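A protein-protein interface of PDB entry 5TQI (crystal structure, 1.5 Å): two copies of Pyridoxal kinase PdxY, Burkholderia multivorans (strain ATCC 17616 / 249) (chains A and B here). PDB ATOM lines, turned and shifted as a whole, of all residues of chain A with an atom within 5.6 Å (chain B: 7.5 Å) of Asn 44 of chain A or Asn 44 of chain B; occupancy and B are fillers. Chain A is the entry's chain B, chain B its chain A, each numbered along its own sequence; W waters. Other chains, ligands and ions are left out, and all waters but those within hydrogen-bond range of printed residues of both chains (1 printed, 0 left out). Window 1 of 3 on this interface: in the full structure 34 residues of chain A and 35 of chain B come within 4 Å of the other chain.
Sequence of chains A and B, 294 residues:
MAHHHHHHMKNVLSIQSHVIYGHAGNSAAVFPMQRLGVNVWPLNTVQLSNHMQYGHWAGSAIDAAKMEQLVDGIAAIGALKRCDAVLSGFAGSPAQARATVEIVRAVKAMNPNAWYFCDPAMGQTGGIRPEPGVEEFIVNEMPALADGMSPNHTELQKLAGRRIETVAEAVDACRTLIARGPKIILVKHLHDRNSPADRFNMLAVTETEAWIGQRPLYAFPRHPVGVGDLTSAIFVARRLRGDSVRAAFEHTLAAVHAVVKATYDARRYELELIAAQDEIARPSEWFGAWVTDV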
ATOM      1  N   SER A  14       3.657  29.978 -23.891  1.00  0.00           N
ATOM      2  CA  SER A  14       2.946  30.189 -22.629  1.00  0.00           C
ATOM      3  C   SER A  14       3.705  31.221 -21.807  1.00  0.00           C
ATOM      4  O   SER A  14       4.839  30.972 -21.372  1.00  0.00           O
ATOM      5  CB  SER A  14       2.781  28.884 -21.854  1.00  0.00           C
ATOM      6  OG  SER A  14       2.063  29.112 -20.652  1.00  0.00           O
ATOM      7  N   GLN A  16       3.825  33.147 -18.566  1.00  0.00           N
ATOM      8  CA  GLN A  16       3.321  33.144 -17.199  1.00  0.00           C
ATOM      9  C   GLN A  16       4.490  33.086 -16.227  1.00  0.00           C
ATOM     10  O   GLN A  16       5.654  32.957 -16.621  1.00  0.00           O
ATOM     11  CB  GLN A  16       2.413  31.936 -16.929  1.00  0.00           C
ATOM     12  CG  GLN A  16       1.328  31.690 -17.962  1.00  0.00           C
ATOM     13  CD  GLN A  16       0.326  30.662 -17.520  1.00  0.00           C
ATOM     14  OE1 GLN A  16      -0.192  30.722 -16.401  1.00  0.00           O
ATOM     15  NE2 GLN A  16       0.045  29.702 -18.392  1.00  0.00           N
ATOM     16  N   SER A  17       4.160  33.160 -14.942  1.00  0.00           N
ATOM     17  CA  SER A  17       5.173  33.055 -13.906  1.00  0.00           C
ATOM     18  C   SER A  17       5.714  31.632 -13.832  1.00  0.00           C
ATOM     19  O   SER A  17       5.031  30.662 -14.160  1.00  0.00           O
ATOM     20  CB  SER A  17       4.567  33.438 -12.555  1.00  0.00           C
ATOM     21  OG  SER A  17       4.065  34.769 -12.583  1.00  0.00           O
ATOM     22  N   HIS A  18       6.958  31.515 -13.382  1.00  0.00           N
ATOM     23  CA  HIS A  18       7.551  30.222 -13.073  1.00  0.00           C
ATOM     24  C   HIS A  18       7.724  30.154 -11.565  1.00  0.00           C
ATOM     25  O   HIS A  18       8.177  31.123 -10.952  1.00  0.00           O
ATOM     26  CB  HIS A  18       8.922  30.077 -13.738  1.00  0.00           C
ATOM     27  CG  HIS A  18       9.682  28.862 -13.299  1.00  0.00           C
ATOM     28  ND1 HIS A  18       9.214  27.585 -13.506  1.00  0.00           N
ATOM     29  CD2 HIS A  18      10.872  28.732 -12.662  1.00  0.00           C
ATOM     30  CE1 HIS A  18      10.085  26.716 -13.018  1.00  0.00           C
ATOM     31  NE2 HIS A  18      11.093  27.386 -12.492  1.00  0.00           N
ATOM     32  N   ILE A  20       9.525  27.665  -8.670  1.00  0.00           N
ATOM     33  CA  ILE A  20      10.489  26.566  -8.591  1.00  0.00           C
ATOM     34  C   ILE A  20       9.888  25.385  -7.847  1.00  0.00           C
ATOM     35  O   ILE A  20       9.869  24.254  -8.347  1.00  0.00           O
ATOM     36  CB  ILE A  20      11.800  27.034  -7.936  1.00  0.00           C
ATOM     37  CG1 ILE A  20      12.406  28.190  -8.740  1.00  0.00           C
ATOM     38  CG2 ILE A  20      12.784  25.846  -7.795  1.00  0.00           C
ATOM     39  CD1 ILE A  20      13.491  28.958  -8.013  1.00  0.00           C
ATOM     40  N   ASN A  26       3.263  28.892 -15.091  1.00  0.00           N
ATOM     41  CA  ASN A  26       3.859  27.901 -15.982  1.00  0.00           C
ATOM     42  C   ASN A  26       4.163  26.593 -15.271  1.00  0.00           C
ATOM     43  O   ASN A  26       4.174  25.532 -15.909  1.00  0.00           O
ATOM     44  CB  ASN A  26       5.092  28.471 -16.688  1.00  0.00           C
ATOM     45  CG  ASN A  26       4.728  29.158 -17.989  1.00  0.00           C
ATOM     46  OD1 ASN A  26       3.655  28.909 -18.538  1.00  0.00           O
ATOM     47  ND2 ASN A  26       5.612  30.006 -18.497  1.00  0.00           N
ATOM     48  N   PRO A  42       7.929  27.893 -22.949  1.00  0.00           N
ATOM     49  CA  PRO A  42       7.588  28.678 -21.757  1.00  0.00           C
ATOM     50  C   PRO A  42       8.405  29.951 -21.660  1.00  0.00           C
ATOM     51  O   PRO A  42       9.636  29.903 -21.569  1.00  0.00           O
ATOM     52  CB  PRO A  42       7.913  27.728 -20.588  1.00  0.00           C
ATOM     53  CG  PRO A  42       8.255  26.384 -21.233  1.00  0.00           C
ATOM     54  CD  PRO A  42       8.768  26.737 -22.610  1.00  0.00           C
ATOM     55  N   LEU A  43       7.728  31.091 -21.701  1.00  0.00           N
ATOM     56  CA  LEU A  43       8.349  32.380 -21.428  1.00  0.00           C
ATOM     57  C   LEU A  43       7.983  32.728 -19.992  1.00  0.00           C
ATOM     58  O   LEU A  43       6.818  33.013 -19.694  1.00  0.00           O
ATOM     59  CB  LEU A  43       7.850  33.447 -22.402  1.00  0.00           C
ATOM     60  CG  LEU A  43       8.676  34.732 -22.530  1.00  0.00           C
ATOM     61  CD1 LEU A  43       8.213  35.500 -23.748  1.00  0.00           C
ATOM     62  CD2 LEU A  43       8.587  35.614 -21.286  1.00  0.00           C
ATOM     63  N   ASN A  44       8.968  32.666 -19.102  1.00  0.00           N
ATOM     64  CA  ASN A  44       8.734  32.879 -17.680  1.00  0.00           C
ATOM     65  C   ASN A  44       8.902  34.357 -17.341  1.00  0.00           C
ATOM     66  O   ASN A  44      10.006  34.904 -17.449  1.00  0.00           O
ATOM     67  CB  ASN A  44       9.684  32.024 -16.845  1.00  0.00           C
ATOM     68  CG  ASN A  44       9.544  30.536 -17.129  1.00  0.00           C
ATOM     69  OD1 ASN A  44       8.442  30.025 -17.346  1.00  0.00           O
ATOM     70  ND2 ASN A  44      10.665  29.829 -17.107  1.00  0.00           N
ATOM     71  N   THR A  45       7.811  34.995 -16.912  1.00  0.00           N
ATOM     72  CA  THR A  45       7.838  36.427 -16.625  1.00  0.00           C
ATOM     73  C   THR A  45       8.526  36.728 -15.302  1.00  0.00           C
ATOM     74  O   THR A  45       9.085  37.820 -15.128  1.00  0.00           O
ATOM     75  CB  THR A  45       6.413  36.965 -16.574  1.00  0.00           C
ATOM     76  OG1 THR A  45       5.645  36.146 -15.677  1.00  0.00           O
ATOM     77  CG2 THR A  45       5.770  36.950 -17.970  1.00  0.00           C
ATOM     78  N   VAL A  46       8.456  35.792 -14.356  1.00  0.00           N
ATOM     79  CA  VAL A  46       9.168  35.869 -13.090  1.00  0.00           C
ATOM     80  C   VAL A  46       9.560  34.450 -12.719  1.00  0.00           C
ATOM     81  O   VAL A  46       9.030  33.475 -13.256  1.00  0.00           O
ATOM     82  CB  VAL A  46       8.320  36.474 -11.945  1.00  0.00           C
ATOM     83  CG1 VAL A  46       7.896  37.889 -12.245  1.00  0.00           C
ATOM     84  CG2 VAL A  46       7.127  35.604 -11.651  1.00  0.00           C
ATOM     85  N   GLN A  47      10.502  34.340 -11.786  1.00  0.00           N
ATOM     86  CA  GLN A  47      10.861  33.060 -11.182  1.00  0.00           C
ATOM     87  C   GLN A  47      10.744  33.221  -9.673  1.00  0.00           C
ATOM     88  O   GLN A  47      11.505  33.979  -9.066  1.00  0.00           O
ATOM     89  CB  GLN A  47      12.277  32.662 -11.578  1.00  0.00           C
ATOM     90  CG  GLN A  47      12.801  31.460 -10.846  1.00  0.00           C
ATOM     91  CD  GLN A  47      14.004  30.828 -11.535  1.00  0.00           C
ATOM     92  OE1 GLN A  47      14.065  29.611 -11.698  1.00  0.00           O
ATOM     93  NE2 GLN A  47      14.958  31.648 -11.947  1.00  0.00           N
ATOM     94  N   ILE A  62      11.781  39.540 -14.988  1.00  0.00           N
ATOM     95  CA  ILE A  62      12.196  40.254 -16.185  1.00  0.00           C
ATOM     96  C   ILE A  62      11.198  41.374 -16.453  1.00  0.00           C
ATOM     97  O   ILE A  62      10.050  41.345 -15.996  1.00  0.00           O
ATOM     98  CB  ILE A  62      12.366  39.336 -17.415  1.00  0.00           C
ATOM     99  CG1 ILE A  62      11.035  38.699 -17.811  1.00  0.00           C
ATOM    100  CG2 ILE A  62      13.403  38.257 -17.140  1.00  0.00           C
ATOM    101  CD1 ILE A  62      11.118  37.883 -19.101  1.00  0.00           C
ATOM    102  N   SER B  14      16.711  20.887 -10.031  1.00  0.00           N
ATOM    103  CA  SER B  14      17.456  20.856 -11.290  1.00  0.00           C
ATOM    104  C   SER B  14      17.900  22.277 -11.615  1.00  0.00           C
ATOM    105  O   SER B  14      17.066  23.136 -11.931  1.00  0.00           O
ATOM    106  CB  SER B  14      16.609  20.270 -12.420  1.00  0.00           C
ATOM    107  OG  SER B  14      17.340  20.233 -13.636  1.00  0.00           O
ATOM    108  N   ILE B  15      19.209  22.516 -11.535  1.00  0.00           N
ATOM    109  CA  ILE B  15      19.801  23.848 -11.618  1.00  0.00           C
ATOM    110  C   ILE B  15      20.471  23.947 -12.981  1.00  0.00           C
ATOM    111  O   ILE B  15      21.592  23.466 -13.165  1.00  0.00           O
ATOM    112  CB  ILE B  15      20.812  24.081 -10.492  1.00  0.00           C
ATOM    113  CG1 ILE B  15      20.186  23.787  -9.120  1.00  0.00           C
ATOM    114  CG2 ILE B  15      21.350  25.497 -10.566  1.00  0.00           C
ATOM    115  CD1 ILE B  15      21.189  23.866  -7.961  1.00  0.00           C
ATOM    116  N   GLN B  16      19.775  24.538 -13.954  1.00  0.00           N
ATOM    117  CA  GLN B  16      20.228  24.523 -15.334  1.00  0.00           C
ATOM    118  C   GLN B  16      19.690  25.758 -16.041  1.00  0.00           C
ATOM    119  O   GLN B  16      18.885  26.510 -15.496  1.00  0.00           O
ATOM    120  CB  GLN B  16      19.723  23.274 -16.080  1.00  0.00           C
ATOM    121  CG  GLN B  16      20.038  21.944 -15.417  1.00  0.00           C
ATOM    122  CD  GLN B  16      19.979  20.790 -16.374  1.00  0.00           C
ATOM    123  OE1 GLN B  16      20.476  20.871 -17.502  1.00  0.00           O
ATOM    124  NE2 GLN B  16      19.371  19.701 -15.938  1.00  0.00           N
ATOM    125  N   SER B  17      20.136  25.948 -17.280  1.00  0.00           N
ATOM    126  CA  SER B  17      19.565  26.979 -18.128  1.00  0.00           C
ATOM    127  C   SER B  17      18.146  26.600 -18.535  1.00  0.00           C
ATOM    128  O   SER B  17      17.734  25.442 -18.455  1.00  0.00           O
ATOM    129  CB  SER B  17      20.392  27.108 -19.399  1.00  0.00           C
ATOM    130  OG  SER B  17      20.410  25.865 -20.083  1.00  0.00           O
ATOM    131  N   HIS B  18      17.388  27.597 -18.971  1.00  0.00           N
ATOM    132  CA  HIS B  18      16.071  27.380 -19.552  1.00  0.00           C
ATOM    133  C   HIS B  18      16.079  27.996 -20.938  1.00  0.00           C
ATOM    134  O   HIS B  18      16.539  29.127 -21.108  1.00  0.00           O
ATOM    135  CB  HIS B  18      14.979  28.050 -18.718  1.00  0.00           C
ATOM    136  CG  HIS B  18      13.634  28.046 -19.376  1.00  0.00           C
ATOM    137  ND1 HIS B  18      12.937  26.885 -19.640  1.00  0.00           N
ATOM    138  CD2 HIS B  18      12.869  29.060 -19.846  1.00  0.00           C
ATOM    139  CE1 HIS B  18      11.796  27.188 -20.236  1.00  0.00           C
ATOM    140  NE2 HIS B  18      11.731  28.500 -20.373  1.00  0.00           N
ATOM    141  N   VAL B  19      15.580  27.259 -21.927  1.00  0.00           N
ATOM    142  CA  VAL B  19      15.484  27.719 -23.312  1.00  0.00           C
ATOM    143  C   VAL B  19      14.002  27.779 -23.691  1.00  0.00           C
ATOM    144  O   VAL B  19      13.308  26.758 -23.603  1.00  0.00           O
ATOM    145  CB  VAL B  19      16.245  26.760 -24.241  1.00  0.00           C
ATOM    146  CG1 VAL B  19      16.438  27.373 -25.586  1.00  0.00           C
ATOM    147  CG2 VAL B  19      17.589  26.381 -23.628  1.00  0.00           C
ATOM    148  N   ILE B  20      13.523  28.949 -24.114  1.00  0.00           N
ATOM    149  CA  ILE B  20      12.098  29.110 -24.397  1.00  0.00           C
ATOM    150  C   ILE B  20      11.687  28.261 -25.594  1.00  0.00           C
ATOM    151  O   ILE B  20      10.754  27.449 -25.516  1.00  0.00           O
ATOM    152  CB  ILE B  20      11.758  30.595 -24.601  1.00  0.00           C
ATOM    153  CG1 ILE B  20      12.074  31.385 -23.328  1.00  0.00           C
ATOM    154  CG2 ILE B  20      10.291  30.759 -24.992  1.00  0.00           C
ATOM    155  CD1 ILE B  20      12.201  32.888 -23.546  1.00  0.00           C
ATOM    156  N   GLY B  25      19.215  22.165 -21.522  1.00  0.00           N
ATOM    157  CA  GLY B  25      19.144  22.436 -20.098  1.00  0.00           C
ATOM    158  C   GLY B  25      17.836  21.938 -19.512  1.00  0.00           C
ATOM    159  O   GLY B  25      17.403  20.812 -19.773  1.00  0.00           O
ATOM    160  N   ASN B  26      17.183  22.785 -18.716  1.00  0.00           N
ATOM    161  CA  ASN B  26      15.927  22.384 -18.099  1.00  0.00           C
ATOM    162  C   ASN B  26      14.832  22.125 -19.129  1.00  0.00           C
ATOM    163  O   ASN B  26      13.905  21.351 -18.850  1.00  0.00           O
ATOM    164  CB  ASN B  26      15.493  23.405 -17.045  1.00  0.00           C
ATOM    165  CG  ASN B  26      16.066  23.095 -15.686  1.00  0.00           C
ATOM    166  OD1 ASN B  26      16.454  21.952 -15.426  1.00  0.00           O
ATOM    167  ND2 ASN B  26      16.126  24.094 -14.807  1.00  0.00           N
ATOM    168  N   SER B  27      14.906  22.737 -20.316  1.00  0.00           N
ATOM    169  CA  SER B  27      13.946  22.456 -21.379  1.00  0.00           C
ATOM    170  C   SER B  27      14.177  21.098 -22.029  1.00  0.00           C
ATOM    171  O   SER B  27      13.362  20.672 -22.860  1.00  0.00           O
ATOM    172  CB  SER B  27      13.978  23.570 -22.426  1.00  0.00           C
ATOM    173  OG  SER B  27      13.605  24.802 -21.837  1.00  0.00           O
ATOM    174  N   VAL B  30      13.580  18.705 -17.554  1.00  0.00           N
ATOM    175  CA  VAL B  30      12.488  18.722 -16.586  1.00  0.00           C
ATOM    176  C   VAL B  30      11.373  17.789 -17.024  1.00  0.00           C
ATOM    177  O   VAL B  30      10.966  16.897 -16.264  1.00  0.00           O
ATOM    178  CB  VAL B  30      11.984  20.156 -16.350  1.00  0.00           C
ATOM    179  CG1 VAL B  30      10.713  20.146 -15.491  1.00  0.00           C
ATOM    180  CG2 VAL B  30      13.065  20.998 -15.698  1.00  0.00           C
ATOM    181  N   TRP B  41      11.967  20.458  -9.270  1.00  0.00           N
ATOM    182  CA  TRP B  41      11.985  21.862  -8.891  1.00  0.00           C
ATOM    183  C   TRP B  41      13.009  22.530  -9.791  1.00  0.00           C
ATOM    184  O   TRP B  41      14.218  22.410  -9.537  1.00  0.00           O
ATOM    185  CB  TRP B  41      12.392  22.000  -7.421  1.00  0.00           C
ATOM    186  CG  TRP B  41      11.511  21.244  -6.478  1.00  0.00           C
ATOM    187  CD1 TRP B  41      10.242  20.796  -6.713  1.00  0.00           C
ATOM    188  CD2 TRP B  41      11.835  20.844  -5.141  1.00  0.00           C
ATOM    189  NE1 TRP B  41       9.760  20.134  -5.606  1.00  0.00           N
ATOM    190  CE2 TRP B  41      10.717  20.151  -4.626  1.00  0.00           C
ATOM    191  CE3 TRP B  41      12.961  21.010  -4.325  1.00  0.00           C
ATOM    192  CZ2 TRP B  41      10.693  19.624  -3.331  1.00  0.00           C
ATOM    193  CZ3 TRP B  41      12.936  20.481  -3.040  1.00  0.00           C
ATOM    194  CH2 TRP B  41      11.810  19.794  -2.557  1.00  0.00           C
ATOM    195  N   PRO B  42      12.599  23.201 -10.869  1.00  0.00           N
ATOM    196  CA  PRO B  42      13.586  23.758 -11.800  1.00  0.00           C
ATOM    197  C   PRO B  42      14.056  25.131 -11.362  1.00  0.00           C
ATOM    198  O   PRO B  42      13.256  26.067 -11.279  1.00  0.00           O
ATOM    199  CB  PRO B  42      12.812  23.856 -13.128  1.00  0.00           C
ATOM    200  CG  PRO B  42      11.479  23.169 -12.886  1.00  0.00           C
ATOM    201  CD  PRO B  42      11.235  23.328 -11.405  1.00  0.00           C
ATOM    202  N   LEU B  43      15.341  25.263 -11.069  1.00  0.00           N
ATOM    203  CA  LEU B  43      15.950  26.562 -10.824  1.00  0.00           C
ATOM    204  C   LEU B  43      16.652  26.954 -12.118  1.00  0.00           C
ATOM    205  O   LEU B  43      17.646  26.330 -12.506  1.00  0.00           O
ATOM    206  CB  LEU B  43      16.930  26.478  -9.655  1.00  0.00           C
ATOM    207  CG  LEU B  43      17.829  27.703  -9.436  1.00  0.00           C
ATOM    208  CD1 LEU B  43      16.986  28.942  -9.196  1.00  0.00           C
ATOM    209  CD2 LEU B  43      18.824  27.477  -8.288  1.00  0.00           C
ATOM    210  N   ASN B  44      16.129  27.978 -12.787  1.00  0.00           N
ATOM    211  CA  ASN B  44      16.654  28.397 -14.080  1.00  0.00           C
ATOM    212  C   ASN B  44      17.710  29.475 -13.860  1.00  0.00           C
ATOM    213  O   ASN B  44      17.397  30.586 -13.418  1.00  0.00           O
ATOM    214  CB  ASN B  44      15.527  28.904 -14.980  1.00  0.00           C
ATOM    215  CG  ASN B  44      14.460  27.854 -15.223  1.00  0.00           C
ATOM    216  OD1 ASN B  44      14.765  26.660 -15.364  1.00  0.00           O
ATOM    217  ND2 ASN B  44      13.207  28.290 -15.285  1.00  0.00           N
ATOM    218  N   THR B  45      18.960  29.153 -14.184  1.00  0.00           N
ATOM    219  CA  THR B  45      20.053  30.100 -14.001  1.00  0.00           C
ATOM    220  C   THR B  45      20.085  31.160 -15.091  1.00  0.00           C
ATOM    221  O   THR B  45      20.685  32.227 -14.895  1.00  0.00           O
ATOM    222  CB  THR B  45      21.379  29.344 -13.973  1.00  0.00           C
ATOM    223  OG1 THR B  45      21.510  28.575 -15.176  1.00  0.00           O
ATOM    224  CG2 THR B  45      21.432  28.411 -12.764  1.00  0.00           C
ATOM    225  N   VAL B  46      19.475  30.877 -16.240  1.00  0.00           N
ATOM    226  CA  VAL B  46      19.341  31.846 -17.317  1.00  0.00           C
ATOM    227  C   VAL B  46      18.128  31.438 -18.132  1.00  0.00           C
ATOM    228  O   VAL B  46      17.748  30.268 -18.166  1.00  0.00           O
ATOM    229  CB  VAL B  46      20.604  31.879 -18.204  1.00  0.00           C
ATOM    230  CG1 VAL B  46      20.796  30.540 -18.890  1.00  0.00           C
ATOM    231  CG2 VAL B  46      20.521  33.005 -19.230  1.00  0.00           C
ATOM    232  N   GLN B  47      17.505  32.417 -18.776  1.00  0.00           N
ATOM    233  CA  GLN B  47      16.423  32.167 -19.717  1.00  0.00           C
ATOM    234  C   GLN B  47      16.876  32.658 -21.082  1.00  0.00           C
ATOM    235  O   GLN B  47      17.138  33.851 -21.255  1.00  0.00           O
ATOM    236  CB  GLN B  47      15.152  32.892 -19.275  1.00  0.00           C
ATOM    237  CG  GLN B  47      14.001  32.744 -20.230  1.00  0.00           C
ATOM    238  CD  GLN B  47      12.671  33.105 -19.602  1.00  0.00           C
ATOM    239  OE1 GLN B  47      11.668  32.445 -19.856  1.00  0.00           O
ATOM    240  NE2 GLN B  47      12.654  34.156 -18.785  1.00  0.00           N
ATOM    241  N   SER B  60      18.321  36.403 -20.484  1.00  0.00           N
ATOM    242  CA  SER B  60      18.336  37.101 -19.209  1.00  0.00           C
ATOM    243  C   SER B  60      18.766  36.102 -18.153  1.00  0.00           C
ATOM    244  O   SER B  60      18.249  34.983 -18.099  1.00  0.00           O
ATOM    245  CB  SER B  60      16.959  37.677 -18.862  1.00  0.00           C
ATOM    246  OG  SER B  60      16.994  38.354 -17.616  1.00  0.00           O
ATOM    247  N   ALA B  61      19.723  36.498 -17.325  1.00  0.00           N
ATOM    248  CA  ALA B  61      20.282  35.611 -16.321  1.00  0.00           C
ATOM    249  C   ALA B  61      20.008  36.150 -14.926  1.00  0.00           C
ATOM    250  O   ALA B  61      19.786  37.346 -14.725  1.00  0.00           O
ATOM    251  CB  ALA B  61      21.796  35.433 -16.514  1.00  0.00           C
ATOM    252  N   ILE B  62      20.018  35.251 -13.955  1.00  0.00           N
ATOM    253  CA  ILE B  62      20.073  35.646 -12.560  1.00  0.00           C
ATOM    254  C   ILE B  62      21.508  35.461 -12.093  1.00  0.00           C
ATOM    255  O   ILE B  62      22.294  34.721 -12.693  1.00  0.00           O
ATOM    256  CB  ILE B  62      19.076  34.873 -11.669  1.00  0.00           C
ATOM    257  CG1 ILE B  62      19.402  33.377 -11.670  1.00  0.00           C
ATOM    258  CG2 ILE B  62      17.650  35.131 -12.136  1.00  0.00           C
ATOM    259  CD1 ILE B  62      18.593  32.574 -10.667  1.00  0.00           C
ATOM    260  N   LYS B  66      21.145  35.755  -6.321  1.00  0.00           N
ATOM    261  CA  LYS B  66      19.736  35.439  -6.513  1.00  0.00           C
ATOM    262  C   LYS B  66      19.494  33.937  -6.424  1.00  0.00           C
ATOM    263  O   LYS B  66      18.476  33.499  -5.874  1.00  0.00           O
ATOM    264  CB  LYS B  66      19.244  35.999  -7.853  1.00  0.00           C
ATOM    265  CG  LYS B  66      17.762  35.755  -8.154  1.00  0.00           C
ATOM    266  CD  LYS B  66      16.830  36.394  -7.123  1.00  0.00           C
ATOM    267  CE  LYS B  66      16.921  37.913  -7.162  1.00  0.00           C
ATOM    268  NZ  LYS B  66      15.975  38.555  -6.199  1.00  0.00           N
ATOM    269  N   MET B  67      20.418  33.129  -6.956  1.00  0.00           N
ATOM    270  CA  MET B  67      20.292  31.683  -6.808  1.00  0.00           C
ATOM    271  C   MET B  67      20.190  31.300  -5.338  1.00  0.00           C
ATOM    272  O   MET B  67      19.328  30.504  -4.950  1.00  0.00           O
ATOM    273  CB  MET B  67      21.493  30.980  -7.441  1.00  0.00           C
ATOM    274  CG  MET B  67      21.525  31.064  -8.954  1.00  0.00           C
ATOM    275  SD  MET B  67      23.042  30.402  -9.648  1.00  0.00           S
ATOM    276  CE  MET B  67      22.977  28.664  -9.164  1.00  0.00           C
ATOM    277  N   LEU B  70      16.770  32.434  -3.870  1.00  0.00           N
ATOM    278  CA  LEU B  70      15.664  31.583  -4.283  1.00  0.00           C
ATOM    279  C   LEU B  70      15.658  30.292  -3.487  1.00  0.00           C
ATOM    280  O   LEU B  70      14.604  29.840  -3.029  1.00  0.00           O
ATOM    281  CB  LEU B  70      15.767  31.297  -5.784  1.00  0.00           C
ATOM    282  CG  LEU B  70      15.451  32.502  -6.682  1.00  0.00           C
ATOM    283  CD1 LEU B  70      15.859  32.219  -8.120  1.00  0.00           C
ATOM    284  CD2 LEU B  70      13.979  32.866  -6.627  1.00  0.00           C
ATOM    285  N   GLN B  96      28.075  31.454 -10.590  1.00  0.00           N
ATOM    286  CA  GLN B  96      26.927  30.554 -10.587  1.00  0.00           C
ATOM    287  C   GLN B  96      27.342  29.135 -10.228  1.00  0.00           C
ATOM    288  O   GLN B  96      26.630  28.445  -9.486  1.00  0.00           O
ATOM    289  CB  GLN B  96      26.236  30.562 -11.946  1.00  0.00           C
ATOM    290  CG  GLN B  96      25.376  31.791 -12.223  1.00  0.00           C
ATOM    291  CD  GLN B  96      24.467  31.591 -13.425  1.00  0.00           C
ATOM    292  OE1 GLN B  96      24.688  30.691 -14.244  1.00  0.00           O
ATOM    293  NE2 GLN B  96      23.430  32.418 -13.532  1.00  0.00           N
HETATM  294  O   HOH W   1      11.018  26.868 -16.573  1.00  0.00           O
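Water W1 bridges the side-chain amide nitrogen (ND2) of Asn 44 of chain B (2.9 Å) and the side-chain amide nitrogen (ND2) of Asn 44 of chain A (3.0 Å).
N of Asn 44 of chain A lies within hydrogen-bond range of OE1 of Gln 47 of chain B (2.8 Å). The backbone NH (N) of Asn 44 of chain B sits at hydrogen-bond distance from the side-chain amide oxygen (OE1) of Gln 47 of chain A, at 2.8 Å. A ring nitrogen (NE2) of His 18 of chain B is in hydrogen-bond range of the backbone carbonyl oxygen (O) of Pro 42 of chain A (2.8 Å). NE2 of His 18 of chain A is in hydrogen-bond range of O of Pro 42 of chain B, 2.8 Å away. ND2 of Asn 44 of chain B sits close to ND2 of Asn 44 of chain A (3.5 Å).
A ring nitrogen (ND1) of His 18 of chain B lies within hydrogen-bond range of the side-chain hydroxyl (OG) of Ser 27 of chain B (3.1 Å). O of Leu 43 of chain A sits at hydrogen-bond distance from ND2 of Asn 26 of chain A. The backbone carbonyl oxygen (O) of Ser 14 of chain B sits at hydrogen-bond distance from the backbone NH (N) of Leu 43 of chain B, 2.9 Å away.
Of chain B, only His 18, Asn 44 and Gln 47 come within 4 Å of Asn 44 of chain A. Ser 14 of chain B touches none of the printed residues of chain A. Ile 15 of chain B touches none of the printed residues of chain A. Printed residues of chain A within 4 Å of Pro 42 of chain B: His 18 (2.8 Å), Ile 20 (3.4 Å) and Gln 47 (3.7 Å). Of chain A, only His 18 (3.5 Å), Asn 44 (3.5 Å) and Gln 47 (2.8 Å) come within 4 Å of Asn 44 of chain B. Of the printed residues of chain A, Gln 47 of chain B touches Pro 42, Leu 43 and Asn 44. Printed residues of chain A within 4 Å of Ser 60 of chain B: Ile 62. The nearest residue of chain B that does not touch Asn 44 of chain A is Ile 20 of chain B (5.4 Å). The nearest printed residue of chain B that does not touch His 18 of chain A is Leu 43 of chain B (5.0 Å).
Among the printed residues, merely in contact across the chains: Ile 20 of chain A with Trp 41 of chain B, Pro 42 of chain A with Ile 20 of chain B, Ile 20 of chain A with Pro 42 of chain B, His 18 of chain A with Asn 44 of chain B, Asn 44 of chain A with His 18 of chain B, Ile 62 of chain A with Ser 60 of chain B, Gln 47 of chain A with Leu 70 of chain B, Gln 47 of chain A with Pro 42 of chain B, Leu 43 of chain A with Gln 47 of chain B, Pro 42 of chain A with Gln 47 of chain B, Gln 47 of chain A with Leu 43 of chain B, Ile 20 of chain A with Leu 43 of chain B, Ile 20 of chain A with Leu 70 of chain B and Gln 47 of chain A with Ile 62 of chain B.
Hydrophobic or aromatic side chains of chain A that line the printed part of chain B: His 18, Ile 20, Pro 42 and Ile 62. Hydrophobic or aromatic side chains of chain B within 4 Å of the printed part of chain A: His 18, Ile 20, Trp 41, Pro 42, Leu 43, Ile 62 and Leu 70. Among the printed residues, 19 pairs touch across the chains. Among the printed residues, no Asp or Glu carboxylate lies within 4 Å of a Lys or Arg side-chain nitrogen of the other chain.
Pro 42 of chain A touches Gln 47 of chain B, and with the chains exchanged Gln 47 of chain A touches Pro 42 of chain B. Asn 44 of chain A touches Gln 47 of chain B, and with the chains exchanged Gln 47 of chain A touches Asn 44 of chain B. Gln 47 of chain A touches Ile 62 of chain B, but with the chains exchanged Ile 62 of chain A does not touch Gln 47 of chain B (4.04 Å). Positions printed for both chains: 14, 16, 17, 18, 20, 26, 42, 43, 44, 45, 46, 47 and 62.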
